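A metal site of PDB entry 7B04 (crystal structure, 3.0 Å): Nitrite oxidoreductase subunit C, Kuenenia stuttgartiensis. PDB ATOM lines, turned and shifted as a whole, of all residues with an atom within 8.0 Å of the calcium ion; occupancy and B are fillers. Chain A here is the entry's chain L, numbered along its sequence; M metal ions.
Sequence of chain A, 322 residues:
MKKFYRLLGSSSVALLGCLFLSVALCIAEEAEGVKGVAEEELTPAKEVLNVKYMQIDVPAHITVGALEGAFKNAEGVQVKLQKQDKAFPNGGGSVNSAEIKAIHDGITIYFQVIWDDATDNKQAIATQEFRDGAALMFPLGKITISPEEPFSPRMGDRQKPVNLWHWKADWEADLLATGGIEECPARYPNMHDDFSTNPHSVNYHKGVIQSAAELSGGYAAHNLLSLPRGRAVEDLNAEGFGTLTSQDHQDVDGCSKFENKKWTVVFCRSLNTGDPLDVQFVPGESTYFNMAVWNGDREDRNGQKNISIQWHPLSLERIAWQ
Within 4 Å of the calcium ion: Asp 117, Thr 119, Asn 121, Asp 132 and Asn 295.
The backbone carbonyl oxygen (O) of Thr 119 binds the calcium ion (2.2 Å). The calcium ion is bound by OD1 of Asn 295, at 2.3 Å. The calcium ion is bound by OD2 of Asp 132, 2.4 Å away. The side-chain carboxylate (OD1) of Asp 132 binds the calcium ion (2.5 Å). OD1 of Asn 121 is bound to the calcium ion (2.5 Å). The calcium ion is bound by OD1 of Asp 117 (2.5 Å). The calcium ion is bound by OG1 of Thr 119, at 2.8 Å. OD2 of Asp 117 is bound to the calcium ion.
OD1 of Asn 295 sits close to N of Asp 297. The guanidinium group (NH1) of Arg 298 sits close to the side-chain amide nitrogen (ND2) of Asn 295, 3.4 Å away. N of Asn 295 sits at hydrogen-bond distance from OD2 of Asp 300. The backbone NH of Gly 296 sits close to the side-chain carboxylate of Asp 132. The indole nitrogen (NE1) of Trp 263 sits close to the side-chain carboxylate (OD2) of Asp 132 (3.2 Å). The backbone NH of Ala 169 sits at hydrogen-bond distance from the backbone carbonyl oxygen of Asp 132, at 3.1 Å. The side-chain amide oxygen (OD1) of Asn 121 sits close to the backbone NH (N) of Asp 297, 3.4 Å away.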
ATOM      1  N   SER A  94      12.692   4.986 -16.332  1.00  0.00           N
ATOM      2  CA  SER A  94      11.561   5.414 -15.501  1.00  0.00           C
ATOM      3  C   SER A  94      11.955   5.460 -14.024  1.00  0.00           C
ATOM      4  O   SER A  94      11.478   6.313 -13.275  1.00  0.00           O
ATOM      5  CB  SER A  94      10.368   4.494 -15.726  1.00  0.00           C
ATOM      6  OG  SER A  94      10.323   4.097 -17.086  1.00  0.00           O
ATOM      7  N   VAL A  95      12.791   4.516 -13.598  1.00  0.00           N
ATOM      8  CA  VAL A  95      13.253   4.442 -12.218  1.00  0.00           C
ATOM      9  C   VAL A  95      14.755   4.708 -12.212  1.00  0.00           C
ATOM     10  O   VAL A  95      15.502   4.165 -13.032  1.00  0.00           O
ATOM     11  CB  VAL A  95      12.926   3.083 -11.572  1.00  0.00           C
ATOM     12  CG1 VAL A  95      13.033   3.175 -10.080  1.00  0.00           C
ATOM     13  CG2 VAL A  95      11.514   2.666 -11.966  1.00  0.00           C
ATOM     14  N   TRP A 115      11.568   1.601  -4.395  1.00  0.00           N
ATOM     15  CA  TRP A 115      11.800   2.488  -5.520  1.00  0.00           C
ATOM     16  C   TRP A 115      10.578   3.365  -5.722  1.00  0.00           C
ATOM     17  O   TRP A 115       9.518   3.152  -5.117  1.00  0.00           O
ATOM     18  CB  TRP A 115      12.153   1.708  -6.796  1.00  0.00           C
ATOM     19  CG  TRP A 115      11.017   0.981  -7.458  1.00  0.00           C
ATOM     20  CD1 TRP A 115      10.198   1.454  -8.442  1.00  0.00           C
ATOM     21  CD2 TRP A 115      10.609  -0.367  -7.198  1.00  0.00           C
ATOM     22  NE1 TRP A 115       9.293   0.481  -8.802  1.00  0.00           N
ATOM     23  CE2 TRP A 115       9.519  -0.634  -8.055  1.00  0.00           C
ATOM     24  CE3 TRP A 115      11.039  -1.361  -6.318  1.00  0.00           C
ATOM     25  CZ2 TRP A 115       8.864  -1.870  -8.064  1.00  0.00           C
ATOM     26  CZ3 TRP A 115      10.387  -2.584  -6.322  1.00  0.00           C
ATOM     27  CH2 TRP A 115       9.305  -2.819  -7.188  1.00  0.00           C
ATOM     28  N   ASP A 116      10.726   4.364  -6.583  1.00  0.00           N
ATOM     29  CA  ASP A 116       9.716   5.391  -6.791  1.00  0.00           C
ATOM     30  C   ASP A 116       9.000   5.128  -8.100  1.00  0.00           C
ATOM     31  O   ASP A 116       9.635   5.005  -9.148  1.00  0.00           O
ATOM     32  CB  ASP A 116      10.335   6.786  -6.839  1.00  0.00           C
ATOM     33  CG  ASP A 116      10.783   7.283  -5.484  1.00  0.00           C
ATOM     34  OD1 ASP A 116      10.138   6.928  -4.473  1.00  0.00           O
ATOM     35  OD2 ASP A 116      11.792   8.023  -5.436  1.00  0.00           O
ATOM     36  N   ASP A 117       7.675   5.036  -8.030  1.00  0.00           N
ATOM     37  CA  ASP A 117       6.929   4.784  -9.251  1.00  0.00           C
ATOM     38  C   ASP A 117       5.530   5.392  -9.158  1.00  0.00           C
ATOM     39  O   ASP A 117       4.796   5.103  -8.211  1.00  0.00           O
ATOM     40  CB  ASP A 117       6.842   3.302  -9.532  1.00  0.00           C
ATOM     41  CG  ASP A 117       6.027   3.032 -10.720  1.00  0.00           C
ATOM     42  OD1 ASP A 117       4.803   3.039 -10.574  1.00  0.00           O
ATOM     43  OD2 ASP A 117       6.615   2.843 -11.807  1.00  0.00           O
ATOM     44  N   ALA A 118       5.162   6.187 -10.166  1.00  0.00           N
ATOM     45  CA  ALA A 118       3.924   6.954 -10.122  1.00  0.00           C
ATOM     46  C   ALA A 118       2.665   6.123 -10.369  1.00  0.00           C
ATOM     47  O   ALA A 118       1.566   6.610 -10.093  1.00  0.00           O
ATOM     48  CB  ALA A 118       3.976   8.095 -11.136  1.00  0.00           C
ATOM     49  N   THR A 119       2.788   4.890 -10.897  1.00  0.00           N
ATOM     50  CA  THR A 119       1.649   4.109 -11.344  1.00  0.00           C
ATOM     51  C   THR A 119       1.730   2.664 -10.872  1.00  0.00           C
ATOM     52  O   THR A 119       2.736   1.999 -11.092  1.00  0.00           O
ATOM     53  CB  THR A 119       1.562   4.106 -12.876  1.00  0.00           C
ATOM     54  OG1 THR A 119       2.688   3.394 -13.409  1.00  0.00           O
ATOM     55  CG2 THR A 119       1.570   5.517 -13.442  1.00  0.00           C
ATOM     56  N   ASP A 120       0.664   2.137 -10.303  1.00  0.00           N
ATOM     57  CA  ASP A 120       0.644   0.718  -9.945  1.00  0.00           C
ATOM     58  C   ASP A 120       0.014  -0.081 -11.093  1.00  0.00           C
ATOM     59  O   ASP A 120      -1.212  -0.146 -11.233  1.00  0.00           O
ATOM     60  CB  ASP A 120      -0.066   0.458  -8.620  1.00  0.00           C
ATOM     61  CG  ASP A 120      -1.466   1.007  -8.572  1.00  0.00           C
ATOM     62  OD1 ASP A 120      -1.826   1.813  -9.457  1.00  0.00           O
ATOM     63  OD2 ASP A 120      -2.211   0.619  -7.643  1.00  0.00           O
ATOM     64  N   ASN A 121       0.863  -0.645 -11.948  1.00  0.00           N
ATOM     65  CA  ASN A 121       0.403  -1.470 -13.066  1.00  0.00           C
ATOM     66  C   ASN A 121       0.464  -2.914 -12.562  1.00  0.00           C
ATOM     67  O   ASN A 121       1.536  -3.538 -12.538  1.00  0.00           O
ATOM     68  CB  ASN A 121       1.263  -1.267 -14.309  1.00  0.00           C
ATOM     69  CG  ASN A 121       1.547   0.204 -14.581  1.00  0.00           C
ATOM     70  OD1 ASN A 121       2.509   0.779 -14.051  1.00  0.00           O
ATOM     71  ND2 ASN A 121       0.733   0.815 -15.425  1.00  0.00           N
ATOM     72  N   LYS A 122      -0.706  -3.466 -12.213  1.00  0.00           N
ATOM     73  CA  LYS A 122      -0.794  -4.772 -11.566  1.00  0.00           C
ATOM     74  C   LYS A 122      -1.559  -5.763 -12.420  1.00  0.00           C
ATOM     75  O   LYS A 122      -2.143  -6.721 -11.899  1.00  0.00           O
ATOM     76  CB  LYS A 122      -1.501  -4.645 -10.208  1.00  0.00           C
ATOM     77  CG  LYS A 122      -1.030  -3.531  -9.288  1.00  0.00           C
ATOM     78  CD  LYS A 122      -2.213  -2.907  -8.577  1.00  0.00           C
ATOM     79  N   PHE A 130       1.312  -3.684 -19.526  1.00  0.00           N
ATOM     80  CA  PHE A 130       2.425  -4.495 -19.046  1.00  0.00           C
ATOM     81  C   PHE A 130       2.520  -4.398 -17.520  1.00  0.00           C
ATOM     82  O   PHE A 130       1.741  -3.689 -16.874  1.00  0.00           O
ATOM     83  CB  PHE A 130       3.725  -4.064 -19.726  1.00  0.00           C
ATOM     84  CG  PHE A 130       3.676  -4.153 -21.225  1.00  0.00           C
ATOM     85  CD1 PHE A 130       4.030  -5.315 -21.886  1.00  0.00           C
ATOM     86  CD2 PHE A 130       3.255  -3.061 -21.980  1.00  0.00           C
ATOM     87  CE1 PHE A 130       3.959  -5.400 -23.266  1.00  0.00           C
ATOM     88  CE2 PHE A 130       3.187  -3.133 -23.355  1.00  0.00           C
ATOM     89  CZ  PHE A 130       3.545  -4.310 -24.000  1.00  0.00           C
ATOM     90  N   ARG A 131       3.495  -5.105 -16.952  1.00  0.00           N
ATOM     91  CA  ARG A 131       3.578  -5.304 -15.521  1.00  0.00           C
ATOM     92  C   ARG A 131       4.636  -4.419 -14.888  1.00  0.00           C
ATOM     93  O   ARG A 131       5.635  -4.062 -15.515  1.00  0.00           O
ATOM     94  CB  ARG A 131       3.888  -6.769 -15.207  1.00  0.00           C
ATOM     95  CG  ARG A 131       5.359  -7.121 -15.401  1.00  0.00           C
ATOM     96  CD  ARG A 131       5.663  -8.592 -15.185  1.00  0.00           C
ATOM     97  NE  ARG A 131       5.189  -9.417 -16.294  1.00  0.00           N
ATOM     98  CZ  ARG A 131       4.167 -10.266 -16.203  1.00  0.00           C
ATOM     99  NH1 ARG A 131       3.525 -10.395 -15.049  1.00  0.00           N
ATOM    100  NH2 ARG A 131       3.790 -10.976 -17.250  1.00  0.00           N
ATOM    101  N   ASP A 132       4.398  -4.051 -13.638  1.00  0.00           N
ATOM    102  CA  ASP A 132       5.456  -3.563 -12.761  1.00  0.00           C
ATOM    103  C   ASP A 132       6.222  -4.761 -12.202  1.00  0.00           C
ATOM    104  O   ASP A 132       5.631  -5.754 -11.802  1.00  0.00           O
ATOM    105  CB  ASP A 132       4.895  -2.715 -11.631  1.00  0.00           C
ATOM    106  CG  ASP A 132       4.518  -1.318 -12.083  1.00  0.00           C
ATOM    107  OD1 ASP A 132       5.131  -0.836 -13.057  1.00  0.00           O
ATOM    108  OD2 ASP A 132       3.633  -0.710 -11.449  1.00  0.00           O
ATOM    109  N   GLY A 133       7.548  -4.651 -12.180  1.00  0.00           N
ATOM    110  CA  GLY A 133       8.358  -5.767 -11.737  1.00  0.00           C
ATOM    111  C   GLY A 133       9.670  -5.323 -11.112  1.00  0.00           C
ATOM    112  O   GLY A 133      10.163  -4.224 -11.357  1.00  0.00           O
ATOM    113  N   ALA A 169       4.019  -7.879 -10.282  1.00  0.00           N
ATOM    114  CA  ALA A 169       2.920  -7.202  -9.600  1.00  0.00           C
ATOM    115  C   ALA A 169       1.585  -7.901  -9.832  1.00  0.00           C
ATOM    116  O   ALA A 169       0.791  -8.075  -8.897  1.00  0.00           O
ATOM    117  CB  ALA A 169       2.845  -5.736 -10.053  1.00  0.00           C
ATOM    118  N   PHE A 258       2.153  -0.990  -2.477  1.00  0.00           N
ATOM    119  CA  PHE A 258       2.254   0.244  -3.248  1.00  0.00           C
ATOM    120  C   PHE A 258       1.626   1.352  -2.406  1.00  0.00           C
ATOM    121  O   PHE A 258       0.467   1.248  -2.010  1.00  0.00           O
ATOM    122  CB  PHE A 258       1.550   0.131  -4.606  1.00  0.00           C
ATOM    123  CG  PHE A 258       1.646   1.385  -5.444  1.00  0.00           C
ATOM    124  CD1 PHE A 258       2.787   1.659  -6.173  1.00  0.00           C
ATOM    125  CD2 PHE A 258       0.587   2.279  -5.502  1.00  0.00           C
ATOM    126  CE1 PHE A 258       2.880   2.802  -6.947  1.00  0.00           C
ATOM    127  CE2 PHE A 258       0.675   3.430  -6.274  1.00  0.00           C
ATOM    128  CZ  PHE A 258       1.822   3.692  -6.996  1.00  0.00           C
ATOM    129  N   TRP A 263       6.899   1.887  -4.579  1.00  0.00           N
ATOM    130  CA  TRP A 263       6.715   0.452  -4.364  1.00  0.00           C
ATOM    131  C   TRP A 263       7.615  -0.042  -3.244  1.00  0.00           C
ATOM    132  O   TRP A 263       8.772   0.371  -3.122  1.00  0.00           O
ATOM    133  CB  TRP A 263       7.036  -0.339  -5.634  1.00  0.00           C
ATOM    134  CG  TRP A 263       5.911  -0.491  -6.598  1.00  0.00           C
ATOM    135  CD1 TRP A 263       5.751   0.175  -7.775  1.00  0.00           C
ATOM    136  CD2 TRP A 263       4.797  -1.393  -6.490  1.00  0.00           C
ATOM    137  NE1 TRP A 263       4.604  -0.248  -8.405  1.00  0.00           N
ATOM    138  CE2 TRP A 263       3.997  -1.198  -7.635  1.00  0.00           C
ATOM    139  CE3 TRP A 263       4.400  -2.327  -5.530  1.00  0.00           C
ATOM    140  CZ2 TRP A 263       2.824  -1.924  -7.847  1.00  0.00           C
ATOM    141  CZ3 TRP A 263       3.231  -3.036  -5.747  1.00  0.00           C
ATOM    142  CH2 TRP A 263       2.457  -2.823  -6.895  1.00  0.00           C
ATOM    143  N   VAL A 293      14.548  -3.103 -12.217  1.00  0.00           N
ATOM    144  CA  VAL A 293      13.178  -2.683 -11.928  1.00  0.00           C
ATOM    145  C   VAL A 293      12.445  -2.423 -13.238  1.00  0.00           C
ATOM    146  O   VAL A 293      13.037  -1.964 -14.222  1.00  0.00           O
ATOM    147  CB  VAL A 293      13.152  -1.425 -11.019  1.00  0.00           C
ATOM    148  CG1 VAL A 293      11.725  -0.919 -10.828  1.00  0.00           C
ATOM    149  CG2 VAL A 293      13.773  -1.733  -9.669  1.00  0.00           C
ATOM    150  N   TRP A 294      11.152  -2.727 -13.249  1.00  0.00           N
ATOM    151  CA  TRP A 294      10.308  -2.527 -14.416  1.00  0.00           C
ATOM    152  C   TRP A 294       9.162  -1.590 -14.097  1.00  0.00           C
ATOM    153  O   TRP A 294       8.608  -1.623 -12.988  1.00  0.00           O
ATOM    154  CB  TRP A 294       9.724  -3.854 -14.909  1.00  0.00           C
ATOM    155  CG  TRP A 294      10.717  -4.766 -15.538  1.00  0.00           C
ATOM    156  CD1 TRP A 294      10.932  -4.968 -16.874  1.00  0.00           C
ATOM    157  CD2 TRP A 294      11.646  -5.621 -14.848  1.00  0.00           C
ATOM    158  NE1 TRP A 294      11.937  -5.885 -17.053  1.00  0.00           N
ATOM    159  CE2 TRP A 294      12.394  -6.304 -15.829  1.00  0.00           C
ATOM    160  CE3 TRP A 294      11.918  -5.867 -13.501  1.00  0.00           C
ATOM    161  CZ2 TRP A 294      13.389  -7.211 -15.500  1.00  0.00           C
ATOM    162  CZ3 TRP A 294      12.913  -6.771 -13.181  1.00  0.00           C
ATOM    163  CH2 TRP A 294      13.629  -7.432 -14.177  1.00  0.00           C
ATOM    164  N   ASN A 295       8.814  -0.746 -15.064  1.00  0.00           N
ATOM    165  CA  ASN A 295       7.624   0.090 -14.990  1.00  0.00           C
ATOM    166  C   ASN A 295       6.755  -0.222 -16.197  1.00  0.00           C
ATOM    167  O   ASN A 295       7.124   0.099 -17.332  1.00  0.00           O
ATOM    168  CB  ASN A 295       7.984   1.569 -14.943  1.00  0.00           C
ATOM    169  CG  ASN A 295       6.785   2.441 -14.641  1.00  0.00           C
ATOM    170  OD1 ASN A 295       5.749   1.945 -14.209  1.00  0.00           O
ATOM    171  ND2 ASN A 295       6.932   3.750 -14.811  1.00  0.00           N
ATOM    172  N   GLY A 296       5.590  -0.824 -15.942  1.00  0.00           N
ATOM    173  CA  GLY A 296       4.673  -1.176 -17.016  1.00  0.00           C
ATOM    174  C   GLY A 296       4.135   0.034 -17.753  1.00  0.00           C
ATOM    175  O   GLY A 296       3.736  -0.066 -18.918  1.00  0.00           O
ATOM    176  N   ASP A 297       4.092   1.180 -17.082  1.00  0.00           N
ATOM    177  CA  ASP A 297       3.554   2.392 -17.689  1.00  0.00           C
ATOM    178  C   ASP A 297       4.359   2.814 -18.914  1.00  0.00           C
ATOM    179  O   ASP A 297       3.794   3.309 -19.888  1.00  0.00           O
ATOM    180  CB  ASP A 297       3.499   3.513 -16.654  1.00  0.00           C
ATOM    181  CG  ASP A 297       2.452   4.557 -16.975  1.00  0.00           C
ATOM    182  OD1 ASP A 297       1.261   4.203 -17.183  1.00  0.00           O
ATOM    183  OD2 ASP A 297       2.822   5.741 -17.021  1.00  0.00           O
ATOM    184  N   ARG A 298       5.674   2.613 -18.874  1.00  0.00           N
ATOM    185  CA  ARG A 298       6.531   2.902 -20.019  1.00  0.00           C
ATOM    186  C   ARG A 298       6.901   1.618 -20.759  1.00  0.00           C
ATOM    187  O   ARG A 298       7.874   1.598 -21.524  1.00  0.00           O
ATOM    188  CB  ARG A 298       7.805   3.605 -19.563  1.00  0.00           C
ATOM    189  CG  ARG A 298       7.533   4.756 -18.655  1.00  0.00           C
ATOM    190  CD  ARG A 298       6.966   5.961 -19.363  1.00  0.00           C
ATOM    191  NE  ARG A 298       7.411   7.205 -18.748  1.00  0.00           N
ATOM    192  CZ  ARG A 298       7.355   7.499 -17.454  1.00  0.00           C
ATOM    193  NH1 ARG A 298       6.771   6.680 -16.556  1.00  0.00           N
ATOM    194  NH2 ARG A 298       7.814   8.663 -17.042  1.00  0.00           N
ATOM    195  N   ASP A 300       7.934  -1.610 -19.839  1.00  0.00           N
ATOM    196  CA  ASP A 300       9.197  -2.285 -19.503  1.00  0.00           C
ATOM    197  C   ASP A 300       8.898  -3.763 -19.342  1.00  0.00           C
ATOM    198  O   ASP A 300       7.995  -4.105 -18.617  1.00  0.00           O
ATOM    199  CB  ASP A 300       9.721  -1.741 -18.179  1.00  0.00           C
ATOM    200  CG  ASP A 300      10.414  -0.404 -18.214  1.00  0.00           C
ATOM    201  OD1 ASP A 300      10.789   0.044 -19.278  1.00  0.00           O
ATOM    202  OD2 ASP A 300      10.548   0.175 -17.165  1.00  0.00           O
HETATM  203 CA    CA M   1       4.334   1.404 -12.460  1.00  0.00          CA
